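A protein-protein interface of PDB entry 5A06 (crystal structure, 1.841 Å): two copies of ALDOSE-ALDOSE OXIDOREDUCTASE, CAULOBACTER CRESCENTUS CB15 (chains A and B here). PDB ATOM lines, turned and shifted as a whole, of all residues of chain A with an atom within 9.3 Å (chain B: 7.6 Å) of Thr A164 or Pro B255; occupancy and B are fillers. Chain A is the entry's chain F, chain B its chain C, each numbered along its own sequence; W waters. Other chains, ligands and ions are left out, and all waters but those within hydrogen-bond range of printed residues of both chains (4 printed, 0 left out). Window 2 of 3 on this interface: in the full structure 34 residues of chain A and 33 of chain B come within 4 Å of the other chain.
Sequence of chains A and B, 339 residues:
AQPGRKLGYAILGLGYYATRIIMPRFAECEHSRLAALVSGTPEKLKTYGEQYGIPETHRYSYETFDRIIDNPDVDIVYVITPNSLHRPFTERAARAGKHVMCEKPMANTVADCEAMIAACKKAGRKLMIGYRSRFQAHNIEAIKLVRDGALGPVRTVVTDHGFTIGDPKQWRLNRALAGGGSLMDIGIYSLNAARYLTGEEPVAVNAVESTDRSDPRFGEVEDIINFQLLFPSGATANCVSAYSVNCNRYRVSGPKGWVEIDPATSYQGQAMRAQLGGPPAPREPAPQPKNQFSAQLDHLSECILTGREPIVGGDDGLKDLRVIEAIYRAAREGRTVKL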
ATOM      1  N   HIS A 161     -31.880 -19.838 -15.404  1.00  0.00           N
ATOM      2  CA  HIS A 161     -30.919 -18.774 -15.705  1.00  0.00           C
ATOM      3  C   HIS A 161     -30.030 -19.158 -16.868  1.00  0.00           C
ATOM      4  O   HIS A 161     -29.448 -20.241 -16.891  1.00  0.00           O
ATOM      5  CB  HIS A 161     -30.050 -18.449 -14.491  1.00  0.00           C
ATOM      6  CG  HIS A 161     -30.759 -17.657 -13.437  1.00  0.00           C
ATOM      7  ND1 HIS A 161     -31.564 -18.240 -12.480  1.00  0.00           N
ATOM      8  CD2 HIS A 161     -30.793 -16.325 -13.197  1.00  0.00           C
ATOM      9  CE1 HIS A 161     -32.059 -17.300 -11.693  1.00  0.00           C
ATOM     10  NE2 HIS A 161     -31.605 -16.129 -12.107  1.00  0.00           N
ATOM     11  N   GLY A 162     -29.916 -18.268 -17.839  1.00  0.00           N
ATOM     12  CA  GLY A 162     -29.082 -18.546 -18.988  1.00  0.00           C
ATOM     13  C   GLY A 162     -28.928 -17.295 -19.814  1.00  0.00           C
ATOM     14  O   GLY A 162     -29.731 -16.360 -19.679  1.00  0.00           O
ATOM     15  N   PHE A 163     -27.883 -17.265 -20.638  1.00  0.00           N
ATOM     16  CA  PHE A 163     -27.775 -16.256 -21.684  1.00  0.00           C
ATOM     17  C   PHE A 163     -27.040 -16.850 -22.890  1.00  0.00           C
ATOM     18  O   PHE A 163     -26.357 -17.861 -22.777  1.00  0.00           O
ATOM     19  CB  PHE A 163     -27.099 -14.979 -21.168  1.00  0.00           C
ATOM     20  CG  PHE A 163     -25.615 -15.110 -20.894  1.00  0.00           C
ATOM     21  CD1 PHE A 163     -25.154 -15.622 -19.684  1.00  0.00           C
ATOM     22  CD2 PHE A 163     -24.682 -14.684 -21.836  1.00  0.00           C
ATOM     23  CE1 PHE A 163     -23.782 -15.719 -19.424  1.00  0.00           C
ATOM     24  CE2 PHE A 163     -23.311 -14.782 -21.589  1.00  0.00           C
ATOM     25  CZ  PHE A 163     -22.861 -15.305 -20.389  1.00  0.00           C
ATOM     26  N   THR A 164     -27.234 -16.246 -24.057  1.00  0.00           N
ATOM     27  CA  THR A 164     -26.636 -16.756 -25.285  1.00  0.00           C
ATOM     28  C   THR A 164     -25.210 -16.208 -25.388  1.00  0.00           C
ATOM     29  O   THR A 164     -24.996 -15.091 -25.855  1.00  0.00           O
ATOM     30  CB  THR A 164     -27.483 -16.350 -26.517  1.00  0.00           C
ATOM     31  OG1 THR A 164     -27.806 -14.962 -26.415  1.00  0.00           O
ATOM     32  CG2 THR A 164     -28.770 -17.124 -26.538  1.00  0.00           C
ATOM     33  N   ILE A 165     -24.238 -16.988 -24.918  1.00  0.00           N
ATOM     34  CA  ILE A 165     -22.851 -16.525 -24.834  1.00  0.00           C
ATOM     35  C   ILE A 165     -22.258 -16.408 -26.249  1.00  0.00           C
ATOM     36  O   ILE A 165     -22.698 -17.097 -27.178  1.00  0.00           O
ATOM     37  CB  ILE A 165     -21.996 -17.490 -23.931  1.00  0.00           C
ATOM     38  CG1 ILE A 165     -20.705 -16.808 -23.462  1.00  0.00           C
ATOM     39  CG2 ILE A 165     -21.741 -18.816 -24.643  1.00  0.00           C
ATOM     40  CD1 ILE A 165     -20.096 -17.389 -22.158  1.00  0.00           C
ATOM     41  N   GLY A 166     -21.278 -15.523 -26.411  1.00  0.00           N
ATOM     42  CA  GLY A 166     -20.729 -15.224 -27.721  1.00  0.00           C
ATOM     43  C   GLY A 166     -19.309 -15.713 -27.967  1.00  0.00           C
ATOM     44  O   GLY A 166     -19.086 -16.907 -28.132  1.00  0.00           O
ATOM     45  N   ASP A 167     -18.359 -14.780 -27.969  1.00  0.00           N
ATOM     46  CA  ASP A 167     -16.971 -15.040 -28.352  1.00  0.00           C
ATOM     47  C   ASP A 167     -16.364 -16.295 -27.719  1.00  0.00           C
ATOM     48  O   ASP A 167     -16.160 -16.350 -26.511  1.00  0.00           O
ATOM     49  CB  ASP A 167     -16.110 -13.829 -27.991  1.00  0.00           C
ATOM     50  CG  ASP A 167     -14.694 -13.907 -28.565  1.00  0.00           C
ATOM     51  OD1 ASP A 167     -14.284 -14.954 -29.109  1.00  0.00           O
ATOM     52  OD2 ASP A 167     -13.974 -12.898 -28.455  1.00  0.00           O
ATOM     53  N   GLN A 170     -13.298 -16.037 -25.115  1.00  0.00           N
ATOM     54  CA  GLN A 170     -13.399 -15.376 -23.815  1.00  0.00           C
ATOM     55  C   GLN A 170     -13.115 -16.361 -22.682  1.00  0.00           C
ATOM     56  O   GLN A 170     -13.254 -17.576 -22.855  1.00  0.00           O
ATOM     57  CB  GLN A 170     -14.779 -14.743 -23.638  1.00  0.00           C
ATOM     58  CG  GLN A 170     -15.923 -15.747 -23.498  1.00  0.00           C
ATOM     59  CD  GLN A 170     -17.263 -15.046 -23.426  1.00  0.00           C
ATOM     60  OE1 GLN A 170     -17.656 -14.553 -22.369  1.00  0.00           O
ATOM     61  NE2 GLN A 170     -17.955 -14.963 -24.560  1.00  0.00           N
ATOM     62  N   LEU A 173     -15.304 -19.438 -21.484  1.00  0.00           N
ATOM     63  CA  LEU A 173     -15.383 -20.670 -22.285  1.00  0.00           C
ATOM     64  C   LEU A 173     -14.042 -21.424 -22.300  1.00  0.00           C
ATOM     65  O   LEU A 173     -13.828 -22.347 -23.093  1.00  0.00           O
ATOM     66  CB  LEU A 173     -15.863 -20.339 -23.707  1.00  0.00           C
ATOM     67  CG  LEU A 173     -17.303 -19.789 -23.743  1.00  0.00           C
ATOM     68  CD1 LEU A 173     -17.677 -19.281 -25.141  1.00  0.00           C
ATOM     69  CD2 LEU A 173     -18.325 -20.852 -23.260  1.00  0.00           C
ATOM     70  N   SER A 182     -21.714 -23.121 -18.002  1.00  0.00           N
ATOM     71  CA  SER A 182     -22.861 -22.314 -17.590  1.00  0.00           C
ATOM     72  C   SER A 182     -23.186 -22.400 -16.094  1.00  0.00           C
ATOM     73  O   SER A 182     -23.606 -21.411 -15.511  1.00  0.00           O
ATOM     74  CB  SER A 182     -24.103 -22.702 -18.404  1.00  0.00           C
ATOM     75  OG  SER A 182     -24.566 -23.994 -18.026  1.00  0.00           O
ATOM     76  N   ASP A 185     -21.145 -19.910 -13.998  1.00  0.00           N
ATOM     77  CA  ASP A 185     -21.339 -18.486 -14.278  1.00  0.00           C
ATOM     78  C   ASP A 185     -22.745 -17.953 -14.018  1.00  0.00           C
ATOM     79  O   ASP A 185     -22.903 -16.872 -13.436  1.00  0.00           O
ATOM     80  CB  ASP A 185     -20.975 -18.183 -15.734  1.00  0.00           C
ATOM     81  CG  ASP A 185     -21.132 -16.713 -16.063  1.00  0.00           C
ATOM     82  OD1 ASP A 185     -20.296 -15.921 -15.578  1.00  0.00           O
ATOM     83  OD2 ASP A 185     -22.100 -16.344 -16.775  1.00  0.00           O
ATOM     84  N   ILE A 186     -23.761 -18.692 -14.464  1.00  0.00           N
ATOM     85  CA  ILE A 186     -25.126 -18.171 -14.512  1.00  0.00           C
ATOM     86  C   ILE A 186     -26.110 -19.172 -13.870  1.00  0.00           C
ATOM     87  O   ILE A 186     -27.065 -18.778 -13.192  1.00  0.00           O
ATOM     88  CB  ILE A 186     -25.520 -17.805 -15.985  1.00  0.00           C
ATOM     89  CG1 ILE A 186     -26.921 -17.213 -16.064  1.00  0.00           C
ATOM     90  CG2 ILE A 186     -25.369 -19.006 -16.934  1.00  0.00           C
ATOM     91  CD1 ILE A 186     -27.097 -15.901 -15.299  1.00  0.00           C
ATOM     92  N   ASP A 215     -20.076 -27.173 -31.680  1.00  0.00           N
ATOM     93  CA  ASP A 215     -20.233 -25.720 -31.561  1.00  0.00           C
ATOM     94  C   ASP A 215     -18.883 -25.122 -31.166  1.00  0.00           C
ATOM     95  O   ASP A 215     -18.250 -25.590 -30.218  1.00  0.00           O
ATOM     96  CB  ASP A 215     -21.320 -25.388 -30.515  1.00  0.00           C
ATOM     97  CG  ASP A 215     -21.725 -23.905 -30.482  1.00  0.00           C
ATOM     98  OD1 ASP A 215     -20.865 -22.997 -30.474  1.00  0.00           O
ATOM     99  OD2 ASP A 215     -22.943 -23.645 -30.414  1.00  0.00           O
ATOM    100  N   ARG A 217     -18.133 -22.635 -29.528  1.00  0.00           N
ATOM    101  CA  ARG A 217     -18.086 -22.102 -28.168  1.00  0.00           C
ATOM    102  C   ARG A 217     -17.783 -23.162 -27.120  1.00  0.00           C
ATOM    103  O   ARG A 217     -17.245 -22.857 -26.057  1.00  0.00           O
ATOM    104  CB  ARG A 217     -19.408 -21.420 -27.825  1.00  0.00           C
ATOM    105  CG  ARG A 217     -19.668 -20.154 -28.620  1.00  0.00           C
ATOM    106  CD  ARG A 217     -21.082 -19.635 -28.363  1.00  0.00           C
ATOM    107  NE  ARG A 217     -22.081 -20.540 -28.930  1.00  0.00           N
ATOM    108  CZ  ARG A 217     -23.387 -20.480 -28.678  1.00  0.00           C
ATOM    109  NH1 ARG A 217     -23.878 -19.550 -27.865  1.00  0.00           N
ATOM    110  NH2 ARG A 217     -24.202 -21.362 -29.238  1.00  0.00           N
ATOM    111  N   PHE A 218     -18.130 -24.409 -27.412  1.00  0.00           N
ATOM    112  CA  PHE A 218     -18.225 -25.423 -26.359  1.00  0.00           C
ATOM    113  C   PHE A 218     -17.244 -26.594 -26.497  1.00  0.00           C
ATOM    114  O   PHE A 218     -17.610 -27.748 -26.275  1.00  0.00           O
ATOM    115  CB  PHE A 218     -19.668 -25.941 -26.305  1.00  0.00           C
ATOM    116  CG  PHE A 218     -20.693 -24.851 -26.090  1.00  0.00           C
ATOM    117  CD1 PHE A 218     -20.557 -23.945 -25.038  1.00  0.00           C
ATOM    118  CD2 PHE A 218     -21.771 -24.716 -26.948  1.00  0.00           C
ATOM    119  CE1 PHE A 218     -21.490 -22.934 -24.840  1.00  0.00           C
ATOM    120  CE2 PHE A 218     -22.722 -23.700 -26.761  1.00  0.00           C
ATOM    121  CZ  PHE A 218     -22.579 -22.803 -25.707  1.00  0.00           C
ATOM    122  N   ASP A 223     -22.613 -26.400 -22.009  1.00  0.00           N
ATOM    123  CA  ASP A 223     -23.664 -25.462 -22.392  1.00  0.00           C
ATOM    124  C   ASP A 223     -24.847 -25.547 -21.415  1.00  0.00           C
ATOM    125  O   ASP A 223     -25.000 -24.696 -20.529  1.00  0.00           O
ATOM    126  CB  ASP A 223     -24.114 -25.748 -23.842  1.00  0.00           C
ATOM    127  CG  ASP A 223     -25.317 -24.912 -24.265  1.00  0.00           C
ATOM    128  OD1 ASP A 223     -25.647 -23.943 -23.554  1.00  0.00           O
ATOM    129  OD2 ASP A 223     -25.929 -25.238 -25.309  1.00  0.00           O
ATOM    130  N   ILE A 224     -25.668 -26.583 -21.564  1.00  0.00           N
ATOM    131  CA  ILE A 224     -26.832 -26.776 -20.703  1.00  0.00           C
ATOM    132  C   ILE A 224     -26.546 -27.843 -19.655  1.00  0.00           C
ATOM    133  O   ILE A 224     -26.052 -28.935 -19.966  1.00  0.00           O
ATOM    134  CB  ILE A 224     -28.077 -27.190 -21.522  1.00  0.00           C
ATOM    135  CG1 ILE A 224     -28.547 -26.033 -22.405  1.00  0.00           C
ATOM    136  CG2 ILE A 224     -29.223 -27.661 -20.592  1.00  0.00           C
ATOM    137  CD1 ILE A 224     -29.642 -26.422 -23.382  1.00  0.00           C
ATOM    138  N   ALA A 242     -27.906 -22.435 -18.591  1.00  0.00           N
ATOM    139  CA  ALA A 242     -27.687 -22.522 -20.036  1.00  0.00           C
ATOM    140  C   ALA A 242     -26.776 -21.440 -20.600  1.00  0.00           C
ATOM    141  O   ALA A 242     -26.763 -20.304 -20.123  1.00  0.00           O
ATOM    142  CB  ALA A 242     -29.040 -22.479 -20.771  1.00  0.00           C
ATOM    143  N   TYR A 243     -26.019 -21.806 -21.630  1.00  0.00           N
ATOM    144  CA  TYR A 243     -25.232 -20.835 -22.387  1.00  0.00           C
ATOM    145  C   TYR A 243     -25.795 -20.658 -23.812  1.00  0.00           C
ATOM    146  O   TYR A 243     -25.211 -19.941 -24.636  1.00  0.00           O
ATOM    147  CB  TYR A 243     -23.768 -21.270 -22.445  1.00  0.00           C
ATOM    148  CG  TYR A 243     -22.860 -20.684 -21.377  1.00  0.00           C
ATOM    149  CD1 TYR A 243     -23.235 -19.570 -20.623  1.00  0.00           C
ATOM    150  CD2 TYR A 243     -21.601 -21.234 -21.152  1.00  0.00           C
ATOM    151  CE1 TYR A 243     -22.368 -19.023 -19.666  1.00  0.00           C
ATOM    152  CE2 TYR A 243     -20.739 -20.701 -20.211  1.00  0.00           C
ATOM    153  CZ  TYR A 243     -21.124 -19.601 -19.473  1.00  0.00           C
ATOM    154  OH  TYR A 243     -20.240 -19.086 -18.545  1.00  0.00           O
ATOM    155  N   SER A 244     -26.924 -21.296 -24.108  1.00  0.00           N
ATOM    156  CA  SER A 244     -27.469 -21.231 -25.472  1.00  0.00           C
ATOM    157  C   SER A 244     -28.913 -20.715 -25.587  1.00  0.00           C
ATOM    158  O   SER A 244     -29.472 -20.713 -26.686  1.00  0.00           O
ATOM    159  CB  SER A 244     -27.377 -22.613 -26.145  1.00  0.00           C
ATOM    160  OG  SER A 244     -28.113 -23.602 -25.423  1.00  0.00           O
ATOM    161  N   VAL A 245     -29.517 -20.297 -24.471  1.00  0.00           N
ATOM    162  CA  VAL A 245     -30.816 -19.603 -24.490  1.00  0.00           C
ATOM    163  C   VAL A 245     -30.804 -18.473 -23.467  1.00  0.00           C
ATOM    164  O   VAL A 245     -29.983 -18.468 -22.548  1.00  0.00           O
ATOM    165  CB  VAL A 245     -32.024 -20.523 -24.153  1.00  0.00           C
ATOM    166  CG1 VAL A 245     -32.174 -21.648 -25.170  1.00  0.00           C
ATOM    167  CG2 VAL A 245     -31.899 -21.071 -22.728  1.00  0.00           C
ATOM    168  N   ASN A 246     -31.720 -17.525 -23.614  1.00  0.00           N
ATOM    169  CA  ASN A 246     -31.828 -16.441 -22.638  1.00  0.00           C
ATOM    170  C   ASN A 246     -32.988 -16.674 -21.678  1.00  0.00           C
ATOM    171  O   ASN A 246     -34.125 -16.871 -22.112  1.00  0.00           O
ATOM    172  CB  ASN A 246     -31.984 -15.092 -23.347  1.00  0.00           C
ATOM    173  CG  ASN A 246     -30.727 -14.677 -24.081  1.00  0.00           C
ATOM    174  OD1 ASN A 246     -29.707 -14.410 -23.457  1.00  0.00           O
ATOM    175  ND2 ASN A 246     -30.792 -14.628 -25.412  1.00  0.00           N
ATOM    176  N   CYS A 247     -32.692 -16.675 -20.378  1.00  0.00           N
ATOM    177  CA  CYS A 247     -33.720 -16.790 -19.345  1.00  0.00           C
ATOM    178  C   CYS A 247     -33.218 -16.252 -18.002  1.00  0.00           C
ATOM    179  O   CYS A 247     -32.040 -16.349 -17.670  1.00  0.00           O
ATOM    180  CB  CYS A 247     -34.189 -18.247 -19.187  1.00  0.00           C
ATOM    181  SG  CYS A 247     -32.863 -19.453 -18.995  1.00  0.00           S
ATOM    182  N   ALA B 150     -38.651 -20.395 -35.799  1.00  0.00           N
ATOM    183  CA  ALA B 150     -38.625 -19.062 -35.182  1.00  0.00           C
ATOM    184  C   ALA B 150     -37.751 -19.011 -33.926  1.00  0.00           C
ATOM    185  O   ALA B 150     -37.257 -17.944 -33.563  1.00  0.00           O
ATOM    186  CB  ALA B 150     -40.019 -18.604 -34.852  1.00  0.00           C
ATOM    187  N   LEU B 151     -37.557 -20.158 -33.266  1.00  0.00           N
ATOM    188  CA  LEU B 151     -36.724 -20.219 -32.063  1.00  0.00           C
ATOM    189  C   LEU B 151     -35.321 -20.746 -32.324  1.00  0.00           C
ATOM    190  O   LEU B 151     -34.470 -20.681 -31.435  1.00  0.00           O
ATOM    191  CB  LEU B 151     -37.376 -21.118 -30.989  1.00  0.00           C
ATOM    192  CG  LEU B 151     -38.863 -20.949 -30.702  1.00  0.00           C
ATOM    193  CD1 LEU B 151     -39.236 -21.754 -29.452  1.00  0.00           C
ATOM    194  CD2 LEU B 151     -39.216 -19.491 -30.518  1.00  0.00           C
ATOM    195  N   GLY B 152     -35.084 -21.286 -33.522  1.00  0.00           N
ATOM    196  CA  GLY B 152     -33.896 -22.080 -33.772  1.00  0.00           C
ATOM    197  C   GLY B 152     -34.160 -23.463 -33.192  1.00  0.00           C
ATOM    198  O   GLY B 152     -35.288 -23.748 -32.816  1.00  0.00           O
ATOM    199  N   PRO B 153     -33.130 -24.323 -33.117  1.00  0.00           N
ATOM    200  CA  PRO B 153     -33.273 -25.662 -32.513  1.00  0.00           C
ATOM    201  C   PRO B 153     -33.795 -25.558 -31.083  1.00  0.00           C
ATOM    202  O   PRO B 153     -33.320 -24.694 -30.355  1.00  0.00           O
ATOM    203  CB  PRO B 153     -31.839 -26.219 -32.527  1.00  0.00           C
ATOM    204  CG  PRO B 153     -31.108 -25.395 -33.534  1.00  0.00           C
ATOM    205  CD  PRO B 153     -31.744 -24.039 -33.526  1.00  0.00           C
ATOM    206  N   VAL B 154     -34.751 -26.396 -30.680  1.00  0.00           N
ATOM    207  CA  VAL B 154     -35.237 -26.330 -29.301  1.00  0.00           C
ATOM    208  C   VAL B 154     -34.123 -26.743 -28.340  1.00  0.00           C
ATOM    209  O   VAL B 154     -33.477 -27.783 -28.525  1.00  0.00           O
ATOM    210  CB  VAL B 154     -36.470 -27.227 -29.077  1.00  0.00           C
ATOM    211  CG1 VAL B 154     -36.860 -27.267 -27.587  1.00  0.00           C
ATOM    212  CG2 VAL B 154     -37.632 -26.732 -29.916  1.00  0.00           C
ATOM    213  N   ARG B 155     -33.879 -25.920 -27.325  1.00  0.00           N
ATOM    214  CA  ARG B 155     -32.847 -26.237 -26.339  1.00  0.00           C
ATOM    215  C   ARG B 155     -33.465 -26.632 -24.996  1.00  0.00           C
ATOM    216  O   ARG B 155     -33.030 -27.602 -24.385  1.00  0.00           O
ATOM    217  CB  ARG B 155     -31.891 -25.052 -26.155  1.00  0.00           C
ATOM    218  CG  ARG B 155     -31.117 -24.654 -27.425  1.00  0.00           C
ATOM    219  CD  ARG B 155     -30.225 -25.798 -27.938  1.00  0.00           C
ATOM    220  NE  ARG B 155     -29.145 -26.108 -26.998  1.00  0.00           N
ATOM    221  CZ  ARG B 155     -28.621 -27.321 -26.826  1.00  0.00           C
ATOM    222  NH1 ARG B 155     -29.067 -28.346 -27.546  1.00  0.00           N
ATOM    223  NH2 ARG B 155     -27.644 -27.511 -25.938  1.00  0.00           N
ATOM    224  N   THR B 156     -34.451 -25.861 -24.535  1.00  0.00           N
ATOM    225  CA  THR B 156     -35.147 -26.169 -23.284  1.00  0.00           C
ATOM    226  C   THR B 156     -36.673 -26.079 -23.377  1.00  0.00           C
ATOM    227  O   THR B 156     -37.233 -25.211 -24.058  1.00  0.00           O
ATOM    228  CB  THR B 156     -34.711 -25.229 -22.124  1.00  0.00           C
ATOM    229  OG1 THR B 156     -35.055 -23.875 -22.447  1.00  0.00           O
ATOM    230  CG2 THR B 156     -33.216 -25.327 -21.853  1.00  0.00           C
ATOM    231  N   SER B 253     -37.740 -22.729 -25.430  1.00  0.00           N
ATOM    232  CA  SER B 253     -36.663 -21.770 -25.749  1.00  0.00           C
ATOM    233  C   SER B 253     -35.615 -22.330 -26.708  1.00  0.00           C
ATOM    234  O   SER B 253     -35.270 -23.511 -26.656  1.00  0.00           O
ATOM    235  CB  SER B 253     -35.951 -21.322 -24.461  1.00  0.00           C
ATOM    236  OG  SER B 253     -36.866 -20.840 -23.496  1.00  0.00           O
ATOM    237  N   GLY B 254     -35.096 -21.465 -27.578  1.00  0.00           N
ATOM    238  CA  GLY B 254     -34.002 -21.797 -28.466  1.00  0.00           C
ATOM    239  C   GLY B 254     -33.082 -20.590 -28.585  1.00  0.00           C
ATOM    240  O   GLY B 254     -33.344 -19.553 -27.974  1.00  0.00           O
ATOM    241  N   PRO B 255     -32.008 -20.711 -29.377  1.00  0.00           N
ATOM    242  CA  PRO B 255     -31.014 -19.625 -29.468  1.00  0.00           C
ATOM    243  C   PRO B 255     -31.575 -18.342 -30.047  1.00  0.00           C
ATOM    244  O   PRO B 255     -31.031 -17.276 -29.777  1.00  0.00           O
ATOM    245  CB  PRO B 255     -29.938 -20.192 -30.413  1.00  0.00           C
ATOM    246  CG  PRO B 255     -30.217 -21.646 -30.525  1.00  0.00           C
ATOM    247  CD  PRO B 255     -31.679 -21.838 -30.269  1.00  0.00           C
ATOM    248  N   LYS B 256     -32.639 -18.439 -30.841  1.00  0.00           N
ATOM    249  CA  LYS B 256     -33.243 -17.241 -31.450  1.00  0.00           C
ATOM    250  C   LYS B 256     -34.336 -16.581 -30.603  1.00  0.00           C
ATOM    251  O   LYS B 256     -34.762 -15.470 -30.901  1.00  0.00           O
ATOM    252  CB  LYS B 256     -33.808 -17.586 -32.840  1.00  0.00           C
ATOM    253  CG  LYS B 256     -32.721 -17.880 -33.876  1.00  0.00           C
ATOM    254  CD  LYS B 256     -33.242 -18.562 -35.166  1.00  0.00           C
ATOM    255  CE  LYS B 256     -34.399 -17.838 -35.822  1.00  0.00           C
ATOM    256  NZ  LYS B 256     -34.670 -18.400 -37.204  1.00  0.00           N
ATOM    257  N   GLY B 257     -34.792 -17.245 -29.543  1.00  0.00           N
ATOM    258  CA  GLY B 257     -35.847 -16.674 -28.724  1.00  0.00           C
ATOM    259  C   GLY B 257     -36.703 -17.730 -28.042  1.00  0.00           C
ATOM    260  O   GLY B 257     -36.364 -18.919 -28.079  1.00  0.00           O
ATOM    261  N   TRP B 258     -37.809 -17.297 -27.434  1.00  0.00           N
ATOM    262  CA  TRP B 258     -38.692 -18.220 -26.729  1.00  0.00           C
ATOM    263  C   TRP B 258     -40.161 -17.829 -26.794  1.00  0.00           C
ATOM    264  O   TRP B 258     -40.509 -16.689 -27.091  1.00  0.00           O
ATOM    265  CB  TRP B 258     -38.266 -18.374 -25.257  1.00  0.00           C
ATOM    266  CG  TRP B 258     -38.112 -17.109 -24.409  1.00  0.00           C
ATOM    267  CD1 TRP B 258     -36.934 -16.519 -24.054  1.00  0.00           C
ATOM    268  CD2 TRP B 258     -39.150 -16.346 -23.753  1.00  0.00           C
ATOM    269  NE1 TRP B 258     -37.167 -15.433 -23.232  1.00  0.00           N
ATOM    270  CE2 TRP B 258     -38.516 -15.305 -23.035  1.00  0.00           C
ATOM    271  CE3 TRP B 258     -40.544 -16.431 -23.713  1.00  0.00           C
ATOM    272  CZ2 TRP B 258     -39.230 -14.358 -22.295  1.00  0.00           C
ATOM    273  CZ3 TRP B 258     -41.250 -15.490 -22.973  1.00  0.00           C
ATOM    274  CH2 TRP B 258     -40.590 -14.472 -22.274  1.00  0.00           C
ATOM    275  N   GLN B 275     -40.578 -13.859 -26.781  1.00  0.00           N
ATOM    276  CA  GLN B 275     -39.398 -13.027 -26.936  1.00  0.00           C
ATOM    277  C   GLN B 275     -38.735 -13.474 -28.222  1.00  0.00           C
ATOM    278  O   GLN B 275     -38.030 -14.468 -28.232  1.00  0.00           O
ATOM    279  CB  GLN B 275     -38.469 -13.172 -25.724  1.00  0.00           C
ATOM    280  CG  GLN B 275     -37.313 -12.166 -25.661  1.00  0.00           C
ATOM    281  CD  GLN B 275     -36.144 -12.609 -26.513  1.00  0.00           C
ATOM    282  OE1 GLN B 275     -35.401 -13.520 -26.137  1.00  0.00           O
ATOM    283  NE2 GLN B 275     -35.991 -11.988 -27.683  1.00  0.00           N
HETATM  284  O   HOH W   1     -33.351 -14.973 -26.866  1.00  0.00           O
HETATM  285  O   HOH W   2     -36.075 -18.884 -21.656  1.00  0.00           O
HETATM  286  O   HOH W   3     -33.590 -17.674 -25.816  1.00  0.00           O
HETATM  287  O   HOH W   4     -24.707 -26.775 -27.330  1.00  0.00           O
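N of Arg B155 lies within hydrogen-bond range of O of Ser B253 (2.9 Å).
The side-chain hydroxyl of Ser A182 sits at hydrogen-bond distance from the backbone carbonyl oxygen of Asp A223 (2.6 Å).
N of Phe A163 is in hydrogen-bond range of O of Val A245, at 3.1 Å.
The backbone carbonyl oxygen (O) of Thr B156 sits at hydrogen-bond distance from the backbone NH (N) of Ser B253, 2.9 Å away.
OG of Ser A244 lies within hydrogen-bond range of OD2 of Asp A223 (2.7 Å).
The backbone NH (N) of Thr A164 sits at hydrogen-bond distance from the side-chain amide oxygen (OD1) of Asn A246 (3.1 Å).
Thr A164 touches just one residue of chain B: Pro B255.
Of the printed residues of chain B, Val A245 touches Arg B155 (3.6 Å), Ser B253 (3.8 Å) and Gly B254 (3.7 Å).
Of the printed residues of chain A, Ser B253 touches Val A245 (3.8 Å).
Of chain A, only Thr A164 and Ser A244 come within 4 Å of Pro B255.
Of the printed residues of chain A, Trp B258 touches Asn A246 (3.4 Å).
Gln B275 touches none of the printed residues of chain A.
The nearest printed residue of chain B that does not touch Asn A246 is Gln B275 (4.7 Å).
OG of Ser A244 sits at hydrogen-bond distance from NE of Arg B155.
OD2 of Asp A223 lies within salt-bridge range of NH2 of Arg B155 (2.9 Å).
Of the 14 printed residues of chain B, 5 touch a printed residue of chain A.
Hydrophobic or aromatic side chains of chain B within 4 Å of the printed part of chain A: Pro B255 and Trp B258.
Of the 23 printed residues of chain A, 6 touch a printed residue of chain B.
Among the printed residues, Asp or Glu carboxylates within 4 Å of a Lys or Arg side-chain nitrogen of the other chain: Asp A223 with Arg B155.
Among the printed residues, merely in contact across the chains: Thr A164 with Pro B255, Ile A224 with Arg B155, Ser A244 with Pro B255, Val A245 with Arg B155, Val A245 with Ser B253, Val A245 with Gly B254 and Asn A246 with Trp B258.
No position is printed for both chains.
Water W1 lies within hydrogen-bond range of the side-chain amide oxygen (OE1) of Gln B275 and the side-chain amide nitrogen (ND2) of Asn A246.
Water W2 bridges OG of Ser B253 (2.8 Å) and O of Asn A246 (2.8 Å).
Water W4 lies within hydrogen-bond range of the side-chain carboxylate of Asp A223 (2.8 Å) and the guanidinium group of Arg B155 (3.3 Å).
Water W3 lies within hydrogen-bond range of the backbone carbonyl oxygen (O) of Gly B254 (2.9 Å) and the backbone NH (N) of Asn A246 (2.9 Å).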
